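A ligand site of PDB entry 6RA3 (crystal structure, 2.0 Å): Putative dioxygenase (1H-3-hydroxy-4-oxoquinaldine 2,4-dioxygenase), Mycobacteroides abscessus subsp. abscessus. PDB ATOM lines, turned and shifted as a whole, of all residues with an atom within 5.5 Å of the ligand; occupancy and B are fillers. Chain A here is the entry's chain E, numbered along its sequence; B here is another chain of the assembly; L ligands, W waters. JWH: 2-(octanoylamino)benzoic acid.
NE2 of His 95 is in hydrogen-bond range of O3 of the ligand, at 2.7 Å.
NE2 of His 97 lies within hydrogen-bond range of O2 of the ligand (3.5 Å).
A ring nitrogen (NE2) of His 246 sits at hydrogen-bond distance from an oxygen (O1) of the ligand, 2.6 Å away.
O of Trp 155 sits at hydrogen-bond distance from N of His 246 (2.9 Å).
ND1 of His 33 lies within hydrogen-bond range of NE2 of His 167 (3.0 Å).
A ring nitrogen (NE2) of His 19 of chain B lies within hydrogen-bond range of the guanidinium group of Arg 148 (3.3 Å).
OG of Ser 172 sits at hydrogen-bond distance from O of His 167 (3.2 Å).
The backbone NH (N) of Gly 30 lies within hydrogen-bond range of a ring nitrogen (NE2) of His 33, 2.7 Å away.
Merely in contact with the ligand: Trp 31 (2.9 Å), Ala 32 (3.99 Å), His 33 (3.7 Å), Ala 96 (3.7 Å), Phe 131 (3.3 Å), Ile 138 (3.9 Å), Arg 148 (3.96 Å), Trp 155 (3.3 Å), Val 168 (3.7 Å), Ser 172 (3.8 Å), Trp 180 (3.6 Å), Ala 183 (3.96 Å), Ile 187 (3.7 Å), Phe 247 (3.6 Å) and His 19 of chain B (3.9 Å).
Hydrophobic or aromatic side chains within 4 Å of the ligand: Trp 31, His 33, His 95, Ala 96, His 97, Phe 131, Ile 138, Trp 155, Val 168, Trp 180, Ala 183, Ile 187, His 246, Phe 247 and His 19 of chain B.
Within 4 Å of the ligand: Trp 31, Ala 32, His 33, His 95, Ala 96, His 97, Phe 131, Ile 138, Arg 148, Trp 155, Val 168, Ser 172, Trp 180, Ala 183, Ile 187, His 246, Phe 247 and His 19 of chain B.
The nearest printed residue that does not touch the ligand is Leu 151 (4.2 Å).
Water W1 lies within hydrogen-bond range of O of Ala 32, O of Ser 172 and NE1 of Trp 180.
Water W2 lies within hydrogen-bond range of the indole nitrogen (NE1) of Trp 155 (3.2 Å) and an oxygen (O2) of the ligand (3.3 Å).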
ATOM      1  N   GLY A  30     -28.094  17.490 -17.984  1.00  0.00           N
ATOM      2  CA  GLY A  30     -28.235  17.045 -19.345  1.00  0.00           C
ATOM      3  C   GLY A  30     -29.702  17.067 -19.794  1.00  0.00           C
ATOM      4  O   GLY A  30     -30.581  17.597 -19.126  1.00  0.00           O
ATOM      5  N   TRP A  31     -29.935  16.499 -20.969  1.00  0.00           N
ATOM      6  CA  TRP A  31     -31.308  16.275 -21.423  1.00  0.00           C
ATOM      7  C   TRP A  31     -31.999  15.198 -20.619  1.00  0.00           C
ATOM      8  O   TRP A  31     -31.384  14.213 -20.205  1.00  0.00           O
ATOM      9  CB  TRP A  31     -31.301  15.870 -22.887  1.00  0.00           C
ATOM     10  CG  TRP A  31     -31.040  17.006 -23.771  1.00  0.00           C
ATOM     11  CD1 TRP A  31     -29.833  17.436 -24.204  1.00  0.00           C
ATOM     12  CD2 TRP A  31     -32.016  17.868 -24.342  1.00  0.00           C
ATOM     13  NE1 TRP A  31     -30.000  18.530 -25.022  1.00  0.00           N
ATOM     14  CE2 TRP A  31     -31.335  18.823 -25.100  1.00  0.00           C
ATOM     15  CE3 TRP A  31     -33.406  17.943 -24.249  1.00  0.00           C
ATOM     16  CZ2 TRP A  31     -31.987  19.813 -25.804  1.00  0.00           C
ATOM     17  CZ3 TRP A  31     -34.050  18.923 -24.908  1.00  0.00           C
ATOM     18  CH2 TRP A  31     -33.354  19.849 -25.700  1.00  0.00           C
ATOM     19  N   ALA A  32     -33.291  15.403 -20.361  1.00  0.00           N
ATOM     20  CA  ALA A  32     -34.173  14.382 -19.794  1.00  0.00           C
ATOM     21  C   ALA A  32     -33.874  14.058 -18.351  1.00  0.00           C
ATOM     22  O   ALA A  32     -34.314  13.020 -17.840  1.00  0.00           O
ATOM     23  CB  ALA A  32     -34.180  13.071 -20.597  1.00  0.00           C
ATOM     24  N   HIS A  33     -33.181  14.930 -17.626  1.00  0.00           N
ATOM     25  CA  HIS A  33     -33.199  14.837 -16.185  1.00  0.00           C
ATOM     26  C   HIS A  33     -33.126  16.255 -15.633  1.00  0.00           C
ATOM     27  O   HIS A  33     -33.070  17.232 -16.392  1.00  0.00           O
ATOM     28  CB  HIS A  33     -32.098  13.891 -15.671  1.00  0.00           C
ATOM     29  CG  HIS A  33     -30.716  14.306 -16.000  1.00  0.00           C
ATOM     30  ND1 HIS A  33     -29.615  13.754 -15.383  1.00  0.00           N
ATOM     31  CD2 HIS A  33     -30.240  15.197 -16.890  1.00  0.00           C
ATOM     32  CE1 HIS A  33     -28.513  14.317 -15.857  1.00  0.00           C
ATOM     33  NE2 HIS A  33     -28.868  15.191 -16.774  1.00  0.00           N
ATOM     34  N   HIS A  95     -23.783  19.237 -17.046  1.00  0.00           N
ATOM     35  CA  HIS A  95     -23.641  17.824 -17.359  1.00  0.00           C
ATOM     36  C   HIS A  95     -23.864  17.504 -18.844  1.00  0.00           C
ATOM     37  O   HIS A  95     -24.882  17.886 -19.451  1.00  0.00           O
ATOM     38  CB  HIS A  95     -24.589  17.000 -16.507  1.00  0.00           C
ATOM     39  CG  HIS A  95     -24.567  15.541 -16.884  1.00  0.00           C
ATOM     40  ND1 HIS A  95     -23.512  14.724 -16.567  1.00  0.00           N
ATOM     41  CD2 HIS A  95     -25.417  14.797 -17.624  1.00  0.00           C
ATOM     42  CE1 HIS A  95     -23.739  13.504 -17.048  1.00  0.00           C
ATOM     43  NE2 HIS A  95     -24.901  13.530 -17.679  1.00  0.00           N
ATOM     44  N   ALA A  96     -22.887  16.792 -19.414  1.00  0.00           N
ATOM     45  CA  ALA A  96     -22.929  16.306 -20.784  1.00  0.00           C
ATOM     46  C   ALA A  96     -23.434  17.350 -21.756  1.00  0.00           C
ATOM     47  O   ALA A  96     -22.853  18.424 -21.889  1.00  0.00           O
ATOM     48  CB  ALA A  96     -23.783  15.025 -20.862  1.00  0.00           C
ATOM     49  N   HIS A  97     -24.499  17.047 -22.484  1.00  0.00           N
ATOM     50  CA  HIS A  97     -24.878  17.941 -23.534  1.00  0.00           C
ATOM     51  C   HIS A  97     -25.592  19.188 -23.018  1.00  0.00           C
ATOM     52  O   HIS A  97     -25.867  20.082 -23.807  1.00  0.00           O
ATOM     53  CB  HIS A  97     -25.693  17.175 -24.557  1.00  0.00           C
ATOM     54  CG  HIS A  97     -24.871  16.100 -25.184  1.00  0.00           C
ATOM     55  ND1 HIS A  97     -23.877  16.387 -26.097  1.00  0.00           N
ATOM     56  CD2 HIS A  97     -24.757  14.781 -24.902  1.00  0.00           C
ATOM     57  CE1 HIS A  97     -23.219  15.284 -26.386  1.00  0.00           C
ATOM     58  NE2 HIS A  97     -23.738  14.299 -25.680  1.00  0.00           N
ATOM     59  N   PHE A 131     -22.503   6.915 -31.790  1.00  0.00           N
ATOM     60  CA  PHE A 131     -23.267   7.880 -31.022  1.00  0.00           C
ATOM     61  C   PHE A 131     -24.301   8.542 -31.927  1.00  0.00           C
ATOM     62  O   PHE A 131     -25.482   8.662 -31.559  1.00  0.00           O
ATOM     63  CB  PHE A 131     -22.317   8.913 -30.411  1.00  0.00           C
ATOM     64  CG  PHE A 131     -23.003   9.912 -29.496  1.00  0.00           C
ATOM     65  CD1 PHE A 131     -23.764   9.480 -28.423  1.00  0.00           C
ATOM     66  CD2 PHE A 131     -22.894  11.264 -29.739  1.00  0.00           C
ATOM     67  CE1 PHE A 131     -24.408  10.381 -27.582  1.00  0.00           C
ATOM     68  CE2 PHE A 131     -23.538  12.194 -28.904  1.00  0.00           C
ATOM     69  CZ  PHE A 131     -24.285  11.732 -27.827  1.00  0.00           C
ATOM     70  N   LEU A 135     -28.336   8.868 -31.476  1.00  0.00           N
ATOM     71  CA  LEU A 135     -29.091  10.125 -31.589  1.00  0.00           C
ATOM     72  C   LEU A 135     -30.205  10.010 -32.617  1.00  0.00           C
ATOM     73  O   LEU A 135     -31.266  10.627 -32.459  1.00  0.00           O
ATOM     74  CB  LEU A 135     -28.150  11.272 -31.968  1.00  0.00           C
ATOM     75  CG  LEU A 135     -27.043  11.694 -30.987  1.00  0.00           C
ATOM     76  CD1 LEU A 135     -26.279  12.868 -31.597  1.00  0.00           C
ATOM     77  CD2 LEU A 135     -27.586  12.050 -29.619  1.00  0.00           C
ATOM     78  N   ILE A 138     -33.202   7.629 -31.050  1.00  0.00           N
ATOM     79  CA  ILE A 138     -34.159   8.232 -30.104  1.00  0.00           C
ATOM     80  C   ILE A 138     -35.107   9.186 -30.812  1.00  0.00           C
ATOM     81  O   ILE A 138     -36.052   9.696 -30.187  1.00  0.00           O
ATOM     82  CB  ILE A 138     -33.426   8.910 -28.922  1.00  0.00           C
ATOM     83  CG1 ILE A 138     -32.447  10.013 -29.364  1.00  0.00           C
ATOM     84  CG2 ILE A 138     -32.686   7.872 -28.120  1.00  0.00           C
ATOM     85  CD1 ILE A 138     -31.636  10.681 -28.186  1.00  0.00           C
ATOM     86  N   ARG A 148     -32.719   4.581 -25.993  1.00  0.00           N
ATOM     87  CA  ARG A 148     -32.421   5.038 -24.634  1.00  0.00           C
ATOM     88  C   ARG A 148     -31.744   3.951 -23.816  1.00  0.00           C
ATOM     89  O   ARG A 148     -30.715   4.195 -23.164  1.00  0.00           O
ATOM     90  CB  ARG A 148     -33.691   5.499 -23.930  1.00  0.00           C
ATOM     91  CG  ARG A 148     -33.454   5.916 -22.470  1.00  0.00           C
ATOM     92  CD  ARG A 148     -34.714   6.291 -21.740  1.00  0.00           C
ATOM     93  NE  ARG A 148     -35.667   5.179 -21.751  1.00  0.00           N
ATOM     94  CZ  ARG A 148     -36.894   5.231 -21.226  1.00  0.00           C
ATOM     95  NH1 ARG A 148     -37.324   6.346 -20.628  1.00  0.00           N
ATOM     96  NH2 ARG A 148     -37.662   4.167 -21.303  1.00  0.00           N
ATOM     97  N   LEU A 151     -28.132   3.602 -24.700  1.00  0.00           N
ATOM     98  CA  LEU A 151     -27.335   4.671 -24.105  1.00  0.00           C
ATOM     99  C   LEU A 151     -27.076   4.427 -22.622  1.00  0.00           C
ATOM    100  O   LEU A 151     -25.940   4.540 -22.151  1.00  0.00           O
ATOM    101  CB  LEU A 151     -28.031   6.021 -24.309  1.00  0.00           C
ATOM    102  CG  LEU A 151     -27.968   6.570 -25.730  1.00  0.00           C
ATOM    103  CD1 LEU A 151     -28.855   7.782 -25.851  1.00  0.00           C
ATOM    104  CD2 LEU A 151     -26.525   6.914 -26.150  1.00  0.00           C
ATOM    105  N   VAL A 152     -28.125   4.079 -21.884  1.00  0.00           N
ATOM    106  CA  VAL A 152     -28.009   3.906 -20.443  1.00  0.00           C
ATOM    107  C   VAL A 152     -26.981   2.835 -20.114  1.00  0.00           C
ATOM    108  O   VAL A 152     -26.246   2.929 -19.114  1.00  0.00           O
ATOM    109  CB  VAL A 152     -29.375   3.565 -19.831  1.00  0.00           C
ATOM    110  CG1 VAL A 152     -29.212   3.003 -18.434  1.00  0.00           C
ATOM    111  CG2 VAL A 152     -30.264   4.780 -19.806  1.00  0.00           C
ATOM    112  N   TRP A 155     -23.676   4.215 -20.372  1.00  0.00           N
ATOM    113  CA  TRP A 155     -23.406   5.193 -19.334  1.00  0.00           C
ATOM    114  C   TRP A 155     -23.064   4.557 -18.005  1.00  0.00           C
ATOM    115  O   TRP A 155     -22.253   5.108 -17.250  1.00  0.00           O
ATOM    116  CB  TRP A 155     -24.636   6.079 -19.156  1.00  0.00           C
ATOM    117  CG  TRP A 155     -24.948   6.903 -20.342  1.00  0.00           C
ATOM    118  CD1 TRP A 155     -24.105   7.250 -21.389  1.00  0.00           C
ATOM    119  CD2 TRP A 155     -26.192   7.525 -20.601  1.00  0.00           C
ATOM    120  NE1 TRP A 155     -24.782   8.053 -22.281  1.00  0.00           N
ATOM    121  CE2 TRP A 155     -26.065   8.235 -21.813  1.00  0.00           C
ATOM    122  CE3 TRP A 155     -27.420   7.550 -19.922  1.00  0.00           C
ATOM    123  CZ2 TRP A 155     -27.129   8.948 -22.362  1.00  0.00           C
ATOM    124  CZ3 TRP A 155     -28.453   8.255 -20.461  1.00  0.00           C
ATOM    125  CH2 TRP A 155     -28.307   8.934 -21.676  1.00  0.00           C
ATOM    126  N   HIS A 167     -30.366   7.092  -9.680  1.00  0.00           N
ATOM    127  CA  HIS A 167     -30.645   8.267 -10.496  1.00  0.00           C
ATOM    128  C   HIS A 167     -31.247   7.863 -11.832  1.00  0.00           C
ATOM    129  O   HIS A 167     -32.251   8.437 -12.272  1.00  0.00           O
ATOM    130  CB  HIS A 167     -29.396   9.118 -10.753  1.00  0.00           C
ATOM    131  CG  HIS A 167     -29.700  10.335 -11.559  1.00  0.00           C
ATOM    132  ND1 HIS A 167     -30.376  11.418 -11.041  1.00  0.00           N
ATOM    133  CD2 HIS A 167     -29.474  10.605 -12.865  1.00  0.00           C
ATOM    134  CE1 HIS A 167     -30.523  12.326 -12.004  1.00  0.00           C
ATOM    135  NE2 HIS A 167     -29.979  11.856 -13.110  1.00  0.00           N
ATOM    136  N   VAL A 168     -30.638   6.889 -12.495  1.00  0.00           N
ATOM    137  CA  VAL A 168     -31.055   6.564 -13.855  1.00  0.00           C
ATOM    138  C   VAL A 168     -32.319   5.690 -13.840  1.00  0.00           C
ATOM    139  O   VAL A 168     -33.150   5.757 -14.756  1.00  0.00           O
ATOM    140  CB  VAL A 168     -29.902   5.853 -14.612  1.00  0.00           C
ATOM    141  CG1 VAL A 168     -30.370   5.350 -15.943  1.00  0.00           C
ATOM    142  CG2 VAL A 168     -28.703   6.801 -14.801  1.00  0.00           C
ATOM    143  N   SER A 172     -35.403   9.680 -12.889  1.00  0.00           N
ATOM    144  CA  SER A 172     -35.494  10.359 -14.185  1.00  0.00           C
ATOM    145  C   SER A 172     -36.737   9.959 -14.969  1.00  0.00           C
ATOM    146  O   SER A 172     -36.735  10.004 -16.211  1.00  0.00           O
ATOM    147  CB  SER A 172     -34.234  10.104 -15.016  1.00  0.00           C
ATOM    148  OG  SER A 172     -33.091  10.645 -14.372  1.00  0.00           O
ATOM    149  N   TRP A 180     -36.971  12.958 -25.620  1.00  0.00           N
ATOM    150  CA  TRP A 180     -35.825  12.181 -26.082  1.00  0.00           C
ATOM    151  C   TRP A 180     -35.550  12.413 -27.557  1.00  0.00           C
ATOM    152  O   TRP A 180     -34.388  12.476 -27.978  1.00  0.00           O
ATOM    153  CB  TRP A 180     -36.059  10.694 -25.799  1.00  0.00           C
ATOM    154  CG  TRP A 180     -35.690  10.369 -24.407  1.00  0.00           C
ATOM    155  CD1 TRP A 180     -36.509  10.389 -23.324  1.00  0.00           C
ATOM    156  CD2 TRP A 180     -34.395   9.980 -23.938  1.00  0.00           C
ATOM    157  NE1 TRP A 180     -35.808  10.029 -22.198  1.00  0.00           N
ATOM    158  CE2 TRP A 180     -34.505   9.771 -22.550  1.00  0.00           C
ATOM    159  CE3 TRP A 180     -33.151   9.816 -24.551  1.00  0.00           C
ATOM    160  CZ2 TRP A 180     -33.426   9.390 -21.763  1.00  0.00           C
ATOM    161  CZ3 TRP A 180     -32.072   9.416 -23.759  1.00  0.00           C
ATOM    162  CH2 TRP A 180     -32.221   9.223 -22.389  1.00  0.00           C
ATOM    163  N   ALA A 183     -33.881  15.780 -27.778  1.00  0.00           N
ATOM    164  CA  ALA A 183     -32.459  15.717 -27.414  1.00  0.00           C
ATOM    165  C   ALA A 183     -31.620  15.205 -28.588  1.00  0.00           C
ATOM    166  O   ALA A 183     -30.584  15.791 -28.914  1.00  0.00           O
ATOM    167  CB  ALA A 183     -32.264  14.840 -26.187  1.00  0.00           C
ATOM    168  N   GLY A 184     -32.099  14.144 -29.257  1.00  0.00           N
ATOM    169  CA  GLY A 184     -31.412  13.628 -30.438  1.00  0.00           C
ATOM    170  C   GLY A 184     -31.212  14.654 -31.530  1.00  0.00           C
ATOM    171  O   GLY A 184     -30.126  14.764 -32.102  1.00  0.00           O
ATOM    172  N   ILE A 187     -28.789  17.590 -30.124  1.00  0.00           N
ATOM    173  CA  ILE A 187     -27.408  17.152 -29.969  1.00  0.00           C
ATOM    174  C   ILE A 187     -26.805  16.859 -31.334  1.00  0.00           C
ATOM    175  O   ILE A 187     -25.675  17.259 -31.627  1.00  0.00           O
ATOM    176  CB  ILE A 187     -27.325  15.940 -29.035  1.00  0.00           C
ATOM    177  CG1 ILE A 187     -27.841  16.312 -27.639  1.00  0.00           C
ATOM    178  CG2 ILE A 187     -25.873  15.454 -28.956  1.00  0.00           C
ATOM    179  CD1 ILE A 187     -27.914  15.150 -26.702  1.00  0.00           C
ATOM    180  N   HIS A 246     -20.783   7.608 -16.851  1.00  0.00           N
ATOM    181  CA  HIS A 246     -20.979   8.857 -17.574  1.00  0.00           C
ATOM    182  C   HIS A 246     -21.472   9.985 -16.688  1.00  0.00           C
ATOM    183  O   HIS A 246     -21.729  11.083 -17.210  1.00  0.00           O
ATOM    184  CB  HIS A 246     -21.929   8.547 -18.742  1.00  0.00           C
ATOM    185  CG  HIS A 246     -22.450   9.731 -19.508  1.00  0.00           C
ATOM    186  ND1 HIS A 246     -21.630  10.600 -20.199  1.00  0.00           N
ATOM    187  CD2 HIS A 246     -23.723  10.115 -19.773  1.00  0.00           C
ATOM    188  CE1 HIS A 246     -22.379  11.493 -20.826  1.00  0.00           C
ATOM    189  NE2 HIS A 246     -23.652  11.223 -20.587  1.00  0.00           N
ATOM    190  N   PHE A 247     -21.625   9.758 -15.376  1.00  0.00           N
ATOM    191  CA  PHE A 247     -22.216  10.730 -14.451  1.00  0.00           C
ATOM    192  C   PHE A 247     -21.223  11.060 -13.331  1.00  0.00           C
ATOM    193  O   PHE A 247     -21.499  10.814 -12.140  1.00  0.00           O
ATOM    194  CB  PHE A 247     -23.531  10.203 -13.850  1.00  0.00           C
ATOM    195  CG  PHE A 247     -24.572   9.883 -14.881  1.00  0.00           C
ATOM    196  CD1 PHE A 247     -25.420  10.871 -15.313  1.00  0.00           C
ATOM    197  CD2 PHE A 247     -24.712   8.609 -15.425  1.00  0.00           C
ATOM    198  CE1 PHE A 247     -26.387  10.631 -16.221  1.00  0.00           C
ATOM    199  CE2 PHE A 247     -25.695   8.356 -16.343  1.00  0.00           C
ATOM    200  CZ  PHE A 247     -26.524   9.380 -16.756  1.00  0.00           C
ATOM    201  N   HIS B  19     -37.355   0.905 -14.742  1.00  0.00           N
ATOM    202  CA  HIS B  19     -37.317   0.670 -16.184  1.00  0.00           C
ATOM    203  C   HIS B  19     -37.328  -0.805 -16.580  1.00  0.00           C
ATOM    204  O   HIS B  19     -37.116  -1.111 -17.758  1.00  0.00           O
ATOM    205  CB  HIS B  19     -36.093   1.357 -16.797  1.00  0.00           C
ATOM    206  CG  HIS B  19     -36.281   2.830 -17.027  1.00  0.00           C
ATOM    207  ND1 HIS B  19     -35.903   3.793 -16.109  1.00  0.00           N
ATOM    208  CD2 HIS B  19     -36.808   3.508 -18.073  1.00  0.00           C
ATOM    209  CE1 HIS B  19     -36.185   4.994 -16.584  1.00  0.00           C
ATOM    210  NE2 HIS B  19     -36.747   4.839 -17.772  1.00  0.00           N
HETATM  211  C4  JWH L   1     -29.445  12.388 -23.064  1.00  0.00           C
HETATM  212  C14 JWH L   1     -32.631   7.955 -17.657  1.00  0.00           C
HETATM  213  C5  JWH L   1     -27.943  12.242 -22.799  1.00  0.00           C
HETATM  214  C6  JWH L   1     -27.205  11.940 -23.854  1.00  0.00           C
HETATM  215  C11 JWH L   1     -30.798  11.227 -18.439  1.00  0.00           C
HETATM  216  C7  JWH L   1     -25.732  11.774 -23.543  1.00  0.00           C
HETATM  217  C8  JWH L   1     -27.632  12.414 -20.124  1.00  0.00           C
HETATM  218  C9  JWH L   1     -29.093  12.598 -19.682  1.00  0.00           C
HETATM  219  C10 JWH L   1     -29.350  11.725 -18.453  1.00  0.00           C
HETATM  220  C12 JWH L   1     -30.947   9.933 -17.628  1.00  0.00           C
HETATM  221  C13 JWH L   1     -31.956   9.100 -18.436  1.00  0.00           C
HETATM  222  N1  JWH L   1     -27.198  12.302 -21.498  1.00  0.00           N
HETATM  223  C3  JWH L   1     -29.953  12.248 -24.279  1.00  0.00           C
HETATM  224  C1  JWH L   1     -27.797  11.789 -25.251  1.00  0.00           C
HETATM  225  C15 JWH L   1     -34.080   7.834 -18.150  1.00  0.00           C
HETATM  226  C2  JWH L   1     -29.089  11.919 -25.462  1.00  0.00           C
HETATM  227  O1  JWH L   1     -25.381  12.090 -22.354  1.00  0.00           O
HETATM  228  O2  JWH L   1     -24.936  11.301 -24.407  1.00  0.00           O
HETATM  229  O3  JWH L   1     -26.750  12.332 -19.318  1.00  0.00           O
HETATM  230  O   HOH W   1     -35.607  10.576 -18.948  1.00  0.00           O
HETATM  231  O   HOH W   2     -22.647   8.977 -24.430  1.00  0.00           O
HETATM  232  O   HOH W   3     -27.351  15.287 -22.208  1.00  0.00           O
